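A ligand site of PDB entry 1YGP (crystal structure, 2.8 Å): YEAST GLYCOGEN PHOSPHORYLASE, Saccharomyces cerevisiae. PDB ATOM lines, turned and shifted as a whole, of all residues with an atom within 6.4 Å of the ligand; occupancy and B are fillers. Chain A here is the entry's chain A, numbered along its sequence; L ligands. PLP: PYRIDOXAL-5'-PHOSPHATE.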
ATOM      1  N   LEU A 107      -5.731 -37.429  -1.287  1.00  0.00           N
ATOM      2  CA  LEU A 107      -5.286 -36.313  -0.477  1.00  0.00           C
ATOM      3  C   LEU A 107      -6.542 -35.721   0.112  1.00  0.00           C
ATOM      4  O   LEU A 107      -7.111 -34.730  -0.364  1.00  0.00           O
ATOM      5  CB  LEU A 107      -4.594 -35.230  -1.310  1.00  0.00           C
ATOM      6  CG  LEU A 107      -3.154 -34.807  -1.049  1.00  0.00           C
ATOM      7  CD1 LEU A 107      -3.038 -33.356  -1.498  1.00  0.00           C
ATOM      8  CD2 LEU A 107      -2.773 -34.932   0.403  1.00  0.00           C
ATOM      9  N   ASN A 163      -0.416 -37.462  -1.328  1.00  0.00           N
ATOM     10  CA  ASN A 163       0.679 -36.509  -1.379  1.00  0.00           C
ATOM     11  C   ASN A 163       0.487 -35.413  -2.398  1.00  0.00           C
ATOM     12  O   ASN A 163       0.086 -34.311  -2.046  1.00  0.00           O
ATOM     13  CB  ASN A 163       1.962 -37.249  -1.670  1.00  0.00           C
ATOM     14  CG  ASN A 163       3.151 -36.310  -1.686  1.00  0.00           C
ATOM     15  OD1 ASN A 163       3.373 -35.475  -0.800  1.00  0.00           O
ATOM     16  ND2 ASN A 163       3.975 -36.463  -2.710  1.00  0.00           N
ATOM     17  N   GLY A 164       0.681 -35.650  -3.690  1.00  0.00           N
ATOM     18  CA  GLY A 164       0.532 -34.610  -4.684  1.00  0.00           C
ATOM     19  C   GLY A 164      -0.826 -34.675  -5.350  1.00  0.00           C
ATOM     20  O   GLY A 164      -1.752 -35.374  -4.900  1.00  0.00           O
ATOM     21  N   GLY A 165      -0.871 -33.978  -6.480  1.00  0.00           N
ATOM     22  CA  GLY A 165      -2.056 -33.808  -7.291  1.00  0.00           C
ATOM     23  C   GLY A 165      -2.736 -35.109  -7.660  1.00  0.00           C
ATOM     24  O   GLY A 165      -3.972 -35.133  -7.715  1.00  0.00           O
ATOM     25  N   LEU A 166      -2.022 -36.220  -7.876  1.00  0.00           N
ATOM     26  CA  LEU A 166      -2.683 -37.496  -8.176  1.00  0.00           C
ATOM     27  C   LEU A 166      -3.779 -37.873  -7.167  1.00  0.00           C
ATOM     28  O   LEU A 166      -4.885 -38.258  -7.523  1.00  0.00           O
ATOM     29  CB  LEU A 166      -1.665 -38.605  -8.213  1.00  0.00           C
ATOM     30  CG  LEU A 166      -2.227 -39.968  -8.472  1.00  0.00           C
ATOM     31  CD1 LEU A 166      -2.760 -39.953  -9.875  1.00  0.00           C
ATOM     32  CD2 LEU A 166      -1.183 -41.048  -8.273  1.00  0.00           C
ATOM     33  N   ARG A 168      -4.955 -35.681  -4.859  1.00  0.00           N
ATOM     34  CA  ARG A 168      -5.937 -34.617  -4.729  1.00  0.00           C
ATOM     35  C   ARG A 168      -6.999 -34.782  -5.816  1.00  0.00           C
ATOM     36  O   ARG A 168      -8.159 -34.484  -5.550  1.00  0.00           O
ATOM     37  CB  ARG A 168      -5.228 -33.245  -4.836  1.00  0.00           C
ATOM     38  CG  ARG A 168      -6.109 -32.024  -4.554  1.00  0.00           C
ATOM     39  CD  ARG A 168      -6.711 -32.061  -3.154  1.00  0.00           C
ATOM     40  NE  ARG A 168      -8.095 -31.662  -3.225  1.00  0.00           N
ATOM     41  CZ  ARG A 168      -9.020 -32.017  -2.329  1.00  0.00           C
ATOM     42  NH1 ARG A 168      -8.796 -32.794  -1.266  1.00  0.00           N
ATOM     43  NH2 ARG A 168     -10.243 -31.554  -2.536  1.00  0.00           N
ATOM     44  N   ILE A 516     -11.528 -29.460 -10.263  1.00  0.00           N
ATOM     45  CA  ILE A 516     -11.477 -29.372  -8.816  1.00  0.00           C
ATOM     46  C   ILE A 516     -12.870 -29.147  -8.200  1.00  0.00           C
ATOM     47  O   ILE A 516     -13.771 -28.566  -8.852  1.00  0.00           O
ATOM     48  CB  ILE A 516     -10.541 -28.194  -8.377  1.00  0.00           C
ATOM     49  CG1 ILE A 516     -10.982 -26.907  -9.012  1.00  0.00           C
ATOM     50  CG2 ILE A 516      -9.110 -28.490  -8.750  1.00  0.00           C
ATOM     51  CD1 ILE A 516     -10.433 -25.758  -8.231  1.00  0.00           C
ATOM     52  N   TRP A 521     -12.624 -25.893  -2.667  1.00  0.00           N
ATOM     53  CA  TRP A 521     -11.771 -24.847  -3.164  1.00  0.00           C
ATOM     54  C   TRP A 521     -12.394 -23.464  -3.299  1.00  0.00           C
ATOM     55  O   TRP A 521     -11.622 -22.495  -3.307  1.00  0.00           O
ATOM     56  CB  TRP A 521     -11.173 -25.431  -4.460  1.00  0.00           C
ATOM     57  CG  TRP A 521     -10.280 -26.612  -4.039  1.00  0.00           C
ATOM     58  CD1 TRP A 521     -10.564 -27.905  -4.432  1.00  0.00           C
ATOM     59  CD2 TRP A 521      -9.195 -26.559  -3.188  1.00  0.00           C
ATOM     60  NE1 TRP A 521      -9.669 -28.661  -3.826  1.00  0.00           N
ATOM     61  CE2 TRP A 521      -8.847 -27.911  -3.084  1.00  0.00           C
ATOM     62  CE3 TRP A 521      -8.460 -25.596  -2.489  1.00  0.00           C
ATOM     63  CZ2 TRP A 521      -7.785 -28.314  -2.277  1.00  0.00           C
ATOM     64  CZ3 TRP A 521      -7.394 -25.990  -1.685  1.00  0.00           C
ATOM     65  CH2 TRP A 521      -7.063 -27.347  -1.581  1.00  0.00           C
ATOM     66  N   VAL A 606       3.588 -22.469  -5.024  1.00  0.00           N
ATOM     67  CA  VAL A 606       3.493 -23.558  -4.072  1.00  0.00           C
ATOM     68  C   VAL A 606       3.216 -24.876  -4.813  1.00  0.00           C
ATOM     69  O   VAL A 606       2.129 -25.105  -5.377  1.00  0.00           O
ATOM     70  CB  VAL A 606       2.371 -23.304  -2.999  1.00  0.00           C
ATOM     71  CG1 VAL A 606       2.809 -22.155  -2.126  1.00  0.00           C
ATOM     72  CG2 VAL A 606       1.027 -22.902  -3.605  1.00  0.00           C
ATOM     73  N   LYS A 607       4.249 -25.725  -4.897  1.00  0.00           N
ATOM     74  CA  LYS A 607       4.133 -27.061  -5.466  1.00  0.00           C
ATOM     75  C   LYS A 607       5.427 -27.820  -5.231  1.00  0.00           C
ATOM     76  O   LYS A 607       6.355 -27.297  -4.607  1.00  0.00           O
ATOM     77  CB  LYS A 607       3.877 -27.043  -6.968  1.00  0.00           C
ATOM     78  CG  LYS A 607       4.836 -26.286  -7.871  1.00  0.00           C
ATOM     79  CD  LYS A 607       4.100 -26.010  -9.178  1.00  0.00           C
ATOM     80  CE  LYS A 607       2.909 -25.087  -8.941  1.00  0.00           C
ATOM     81  NZ  LYS A 607       2.017 -25.143 -10.090  1.00  0.00           N
ATOM     82  N   ARG A 608       5.483 -29.051  -5.715  1.00  0.00           N
ATOM     83  CA  ARG A 608       6.617 -29.935  -5.545  1.00  0.00           C
ATOM     84  C   ARG A 608       7.861 -29.281  -6.080  1.00  0.00           C
ATOM     85  O   ARG A 608       7.866 -28.718  -7.165  1.00  0.00           O
ATOM     86  CB  ARG A 608       6.328 -31.226  -6.293  1.00  0.00           C
ATOM     87  CG  ARG A 608       7.405 -32.307  -6.290  1.00  0.00           C
ATOM     88  CD  ARG A 608       6.655 -33.618  -6.373  1.00  0.00           C
ATOM     89  NE  ARG A 608       7.000 -34.360  -7.565  1.00  0.00           N
ATOM     90  CZ  ARG A 608       6.531 -34.052  -8.770  1.00  0.00           C
ATOM     91  NH1 ARG A 608       5.701 -33.023  -8.967  1.00  0.00           N
ATOM     92  NH2 ARG A 608       6.864 -34.831  -9.800  1.00  0.00           N
ATOM     93  N   LYS A 613      10.013 -27.961 -12.477  1.00  0.00           N
ATOM     94  CA  LYS A 613       8.959 -27.030 -12.092  1.00  0.00           C
ATOM     95  C   LYS A 613       9.522 -25.632 -12.061  1.00  0.00           C
ATOM     96  O   LYS A 613       8.795 -24.663 -11.828  1.00  0.00           O
ATOM     97  CB  LYS A 613       8.437 -27.303 -10.704  1.00  0.00           C
ATOM     98  CG  LYS A 613       7.861 -28.659 -10.558  1.00  0.00           C
ATOM     99  CD  LYS A 613       6.473 -28.670 -11.087  1.00  0.00           C
ATOM    100  CE  LYS A 613       5.951 -29.959 -10.545  1.00  0.00           C
ATOM    101  NZ  LYS A 613       4.708 -30.258 -11.210  1.00  0.00           N
ATOM    102  N   TYR A 696       3.575 -27.756   3.587  1.00  0.00           N
ATOM    103  CA  TYR A 696       2.432 -27.337   2.785  1.00  0.00           C
ATOM    104  C   TYR A 696       1.626 -28.576   2.522  1.00  0.00           C
ATOM    105  O   TYR A 696       2.077 -29.527   1.903  1.00  0.00           O
ATOM    106  CB  TYR A 696       2.967 -26.715   1.512  1.00  0.00           C
ATOM    107  CG  TYR A 696       1.983 -26.510   0.367  1.00  0.00           C
ATOM    108  CD1 TYR A 696       1.052 -25.474   0.364  1.00  0.00           C
ATOM    109  CD2 TYR A 696       2.057 -27.400  -0.697  1.00  0.00           C
ATOM    110  CE1 TYR A 696       0.203 -25.332  -0.731  1.00  0.00           C
ATOM    111  CE2 TYR A 696       1.216 -27.272  -1.785  1.00  0.00           C
ATOM    112  CZ  TYR A 696       0.291 -26.234  -1.804  1.00  0.00           C
ATOM    113  OH  TYR A 696      -0.508 -26.108  -2.934  1.00  0.00           O
ATOM    114  N   ASN A 697       0.462 -28.543   3.112  1.00  0.00           N
ATOM    115  CA  ASN A 697      -0.513 -29.586   2.967  1.00  0.00           C
ATOM    116  C   ASN A 697      -1.802 -28.941   2.447  1.00  0.00           C
ATOM    117  O   ASN A 697      -1.792 -27.763   2.050  1.00  0.00           O
ATOM    118  CB  ASN A 697      -0.728 -30.228   4.312  1.00  0.00           C
ATOM    119  CG  ASN A 697      -1.178 -29.253   5.385  1.00  0.00           C
ATOM    120  OD1 ASN A 697      -2.052 -28.388   5.206  1.00  0.00           O
ATOM    121  ND2 ASN A 697      -0.568 -29.359   6.547  1.00  0.00           N
ATOM    122  N   VAL A 698      -2.963 -29.596   2.454  1.00  0.00           N
ATOM    123  CA  VAL A 698      -4.142 -28.994   1.849  1.00  0.00           C
ATOM    124  C   VAL A 698      -4.633 -27.789   2.635  1.00  0.00           C
ATOM    125  O   VAL A 698      -4.950 -26.771   2.036  1.00  0.00           O
ATOM    126  CB  VAL A 698      -5.247 -30.091   1.717  1.00  0.00           C
ATOM    127  CG1 VAL A 698      -6.641 -29.541   1.397  1.00  0.00           C
ATOM    128  CG2 VAL A 698      -4.851 -30.945   0.542  1.00  0.00           C
ATOM    129  N   SER A 699      -4.619 -27.852   3.956  1.00  0.00           N
ATOM    130  CA  SER A 699      -5.155 -26.803   4.796  1.00  0.00           C
ATOM    131  C   SER A 699      -4.390 -25.517   4.588  1.00  0.00           C
ATOM    132  O   SER A 699      -4.977 -24.438   4.432  1.00  0.00           O
ATOM    133  CB  SER A 699      -5.084 -27.321   6.204  1.00  0.00           C
ATOM    134  OG  SER A 699      -5.746 -28.577   6.198  1.00  0.00           O
ATOM    135  N   ALA A 701      -2.868 -24.836   1.834  1.00  0.00           N
ATOM    136  CA  ALA A 701      -3.281 -24.424   0.500  1.00  0.00           C
ATOM    137  C   ALA A 701      -4.673 -23.790   0.537  1.00  0.00           C
ATOM    138  O   ALA A 701      -4.956 -22.924  -0.298  1.00  0.00           O
ATOM    139  CB  ALA A 701      -3.317 -25.620  -0.455  1.00  0.00           C
ATOM    140  N   GLU A 702      -5.549 -24.142   1.485  1.00  0.00           N
ATOM    141  CA  GLU A 702      -6.828 -23.482   1.562  1.00  0.00           C
ATOM    142  C   GLU A 702      -6.660 -22.069   2.119  1.00  0.00           C
ATOM    143  O   GLU A 702      -7.544 -21.263   1.906  1.00  0.00           O
ATOM    144  CB  GLU A 702      -7.786 -24.245   2.452  1.00  0.00           C
ATOM    145  CG  GLU A 702      -8.470 -25.466   1.815  1.00  0.00           C
ATOM    146  CD  GLU A 702      -9.235 -26.332   2.830  1.00  0.00           C
ATOM    147  OE1 GLU A 702      -9.995 -25.816   3.645  1.00  0.00           O
ATOM    148  OE2 GLU A 702      -9.052 -27.546   2.810  1.00  0.00           O
ATOM    149  N   ILE A 705      -4.071 -20.271  -1.305  1.00  0.00           N
ATOM    150  CA  ILE A 705      -4.679 -19.957  -2.585  1.00  0.00           C
ATOM    151  C   ILE A 705      -5.661 -18.758  -2.599  1.00  0.00           C
ATOM    152  O   ILE A 705      -5.414 -17.876  -3.433  1.00  0.00           O
ATOM    153  CB  ILE A 705      -5.303 -21.277  -3.091  1.00  0.00           C
ATOM    154  CG1 ILE A 705      -4.120 -22.057  -3.614  1.00  0.00           C
ATOM    155  CG2 ILE A 705      -6.385 -21.105  -4.149  1.00  0.00           C
ATOM    156  CD1 ILE A 705      -4.284 -23.532  -3.993  1.00  0.00           C
ATOM    157  N   HIS A 713       3.196 -20.584 -12.740  1.00  0.00           N
ATOM    158  CA  HIS A 713       2.987 -21.905 -13.294  1.00  0.00           C
ATOM    159  C   HIS A 713       3.939 -22.001 -14.478  1.00  0.00           C
ATOM    160  O   HIS A 713       3.563 -22.108 -15.630  1.00  0.00           O
ATOM    161  CB  HIS A 713       1.515 -22.026 -13.686  1.00  0.00           C
ATOM    162  CG  HIS A 713       0.626 -22.136 -12.442  1.00  0.00           C
ATOM    163  ND1 HIS A 713       0.529 -23.094 -11.520  1.00  0.00           N
ATOM    164  CD2 HIS A 713      -0.231 -21.136 -12.071  1.00  0.00           C
ATOM    165  CE1 HIS A 713      -0.331 -22.700 -10.604  1.00  0.00           C
ATOM    166  NE2 HIS A 713      -0.790 -21.519 -10.951  1.00  0.00           N
ATOM    167  N   GLY A 723      -2.832 -30.078 -14.290  1.00  0.00           N
ATOM    168  CA  GLY A 723      -2.282 -29.265 -13.227  1.00  0.00           C
ATOM    169  C   GLY A 723      -3.408 -28.609 -12.480  1.00  0.00           C
ATOM    170  O   GLY A 723      -3.833 -27.494 -12.804  1.00  0.00           O
ATOM    171  N   THR A 724      -3.915 -29.290 -11.453  1.00  0.00           N
ATOM    172  CA  THR A 724      -5.076 -28.764 -10.785  1.00  0.00           C
ATOM    173  C   THR A 724      -4.854 -27.581  -9.875  1.00  0.00           C
ATOM    174  O   THR A 724      -5.853 -26.848  -9.773  1.00  0.00           O
ATOM    175  CB  THR A 724      -5.798 -29.903 -10.023  1.00  0.00           C
ATOM    176  OG1 THR A 724      -4.875 -30.799  -9.404  1.00  0.00           O
ATOM    177  CG2 THR A 724      -6.638 -30.665 -11.009  1.00  0.00           C
ATOM    178  N   SER A 725      -3.698 -27.220  -9.292  1.00  0.00           N
ATOM    179  CA  SER A 725      -3.726 -26.059  -8.398  1.00  0.00           C
ATOM    180  C   SER A 725      -3.940 -24.758  -9.159  1.00  0.00           C
ATOM    181  O   SER A 725      -4.522 -23.807  -8.619  1.00  0.00           O
ATOM    182  CB  SER A 725      -2.458 -25.932  -7.590  1.00  0.00           C
ATOM    183  OG  SER A 725      -1.293 -25.981  -8.389  1.00  0.00           O
ATOM    184  N   ASN A 726      -3.561 -24.776 -10.441  1.00  0.00           N
ATOM    185  CA  ASN A 726      -3.757 -23.684 -11.396  1.00  0.00           C
ATOM    186  C   ASN A 726      -5.220 -23.299 -11.371  1.00  0.00           C
ATOM    187  O   ASN A 726      -5.569 -22.151 -11.174  1.00  0.00           O
ATOM    188  CB  ASN A 726      -3.447 -24.092 -12.833  1.00  0.00           C
ATOM    189  CG  ASN A 726      -2.055 -24.618 -13.121  1.00  0.00           C
ATOM    190  OD1 ASN A 726      -1.336 -25.118 -12.252  1.00  0.00           O
ATOM    191  ND2 ASN A 726      -1.484 -24.440 -14.307  1.00  0.00           N
ATOM    192  N   LYS A 728      -7.430 -24.036  -9.084  1.00  0.00           N
ATOM    193  CA  LYS A 728      -7.757 -23.563  -7.731  1.00  0.00           C
ATOM    194  C   LYS A 728      -7.435 -22.094  -7.588  1.00  0.00           C
ATOM    195  O   LYS A 728      -8.146 -21.390  -6.883  1.00  0.00           O
ATOM    196  CB  LYS A 728      -6.969 -24.315  -6.641  1.00  0.00           C
ATOM    197  CG  LYS A 728      -7.304 -25.788  -6.526  1.00  0.00           C
ATOM    198  CD  LYS A 728      -6.294 -26.466  -5.643  1.00  0.00           C
ATOM    199  CE  LYS A 728      -6.409 -27.957  -5.856  1.00  0.00           C
ATOM    200  NZ  LYS A 728      -5.427 -28.541  -4.953  1.00  0.00           N
HETATM  201  N1  PLP L   1      -1.055 -30.539  -3.127  1.00  0.00           N
HETATM  202  C2  PLP L   1      -2.023 -29.806  -2.491  1.00  0.00           C
HETATM  203  C2A PLP L   1      -1.898 -29.600  -1.002  1.00  0.00           C
HETATM  204  C3  PLP L   1      -3.095 -29.307  -3.206  1.00  0.00           C
HETATM  205  O3  PLP L   1      -4.102 -28.634  -2.558  1.00  0.00           O
HETATM  206  C4  PLP L   1      -3.188 -29.516  -4.569  1.00  0.00           C
HETATM  207  C4A PLP L   1      -4.052 -28.754  -5.360  1.00  0.00           C
HETATM  208  C5  PLP L   1      -2.202 -30.274  -5.190  1.00  0.00           C
HETATM  209  C6  PLP L   1      -1.148 -30.770  -4.462  1.00  0.00           C
HETATM  210  C5A PLP L   1      -2.200 -30.469  -6.735  1.00  0.00           C
HETATM  211  O4P PLP L   1      -1.501 -29.376  -7.339  1.00  0.00           O
HETATM  212  P   PLP L   1      -0.431 -29.547  -8.486  1.00  0.00           P
HETATM  213  O1P PLP L   1      -0.789 -30.797  -9.216  1.00  0.00           O
HETATM  214  O2P PLP L   1      -0.786 -28.310  -9.446  1.00  0.00           O
HETATM  215  O3P PLP L   1       0.915 -29.285  -7.925  1.00  0.00           O
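Leu 107 touches the ligand (CD1 to N1, 3.8 Å). Gly 165 touches the ligand. Arg 168 touches the ligand. CH2 of Trp 521 touches O3 of the ligand, 3.4 Å away. Lys 607 touches the ligand (CB to O3P, 3.8 Å). CE2 of Tyr 696 touches C2A of the ligand (3.97 Å). Asn 697 touches the ligand. Val 698 touches the ligand (CG2 to C2A, 3.6 Å). Ala 701 touches the ligand (CB to O3, 3.8 Å). OG1 of Thr 724 touches C5A of the ligand, 3.8 Å away. Of the 25 residues printed, 12 come within 4 Å of the ligand. Along chain A the residues within 4 Å of the ligand span positions 107 to 728. The nearest printed residue that does not touch the ligand is Gly 164 (4.02 Å).
N of Ser 699 sits at hydrogen-bond distance from OD1 of Asn 697 (2.9 Å). NZ of Lys 607 sits at hydrogen-bond distance from ND1 of His 713, 2.9 Å away. O of Leu 107 lies within hydrogen-bond range of NH1 of Arg 168 (2.7 Å).
O2P of the ligand is in hydrogen-bond range of N of Ser 725, at 3.1 Å. The side-chain amino group (NZ) of Lys 728 is covalently linked to a carbon (C4A) of the ligand (1.4 Å). The side-chain hydroxyl (OG) of Ser 725 sits at hydrogen-bond distance from an oxygen (O2P) of the ligand (2.6 Å).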
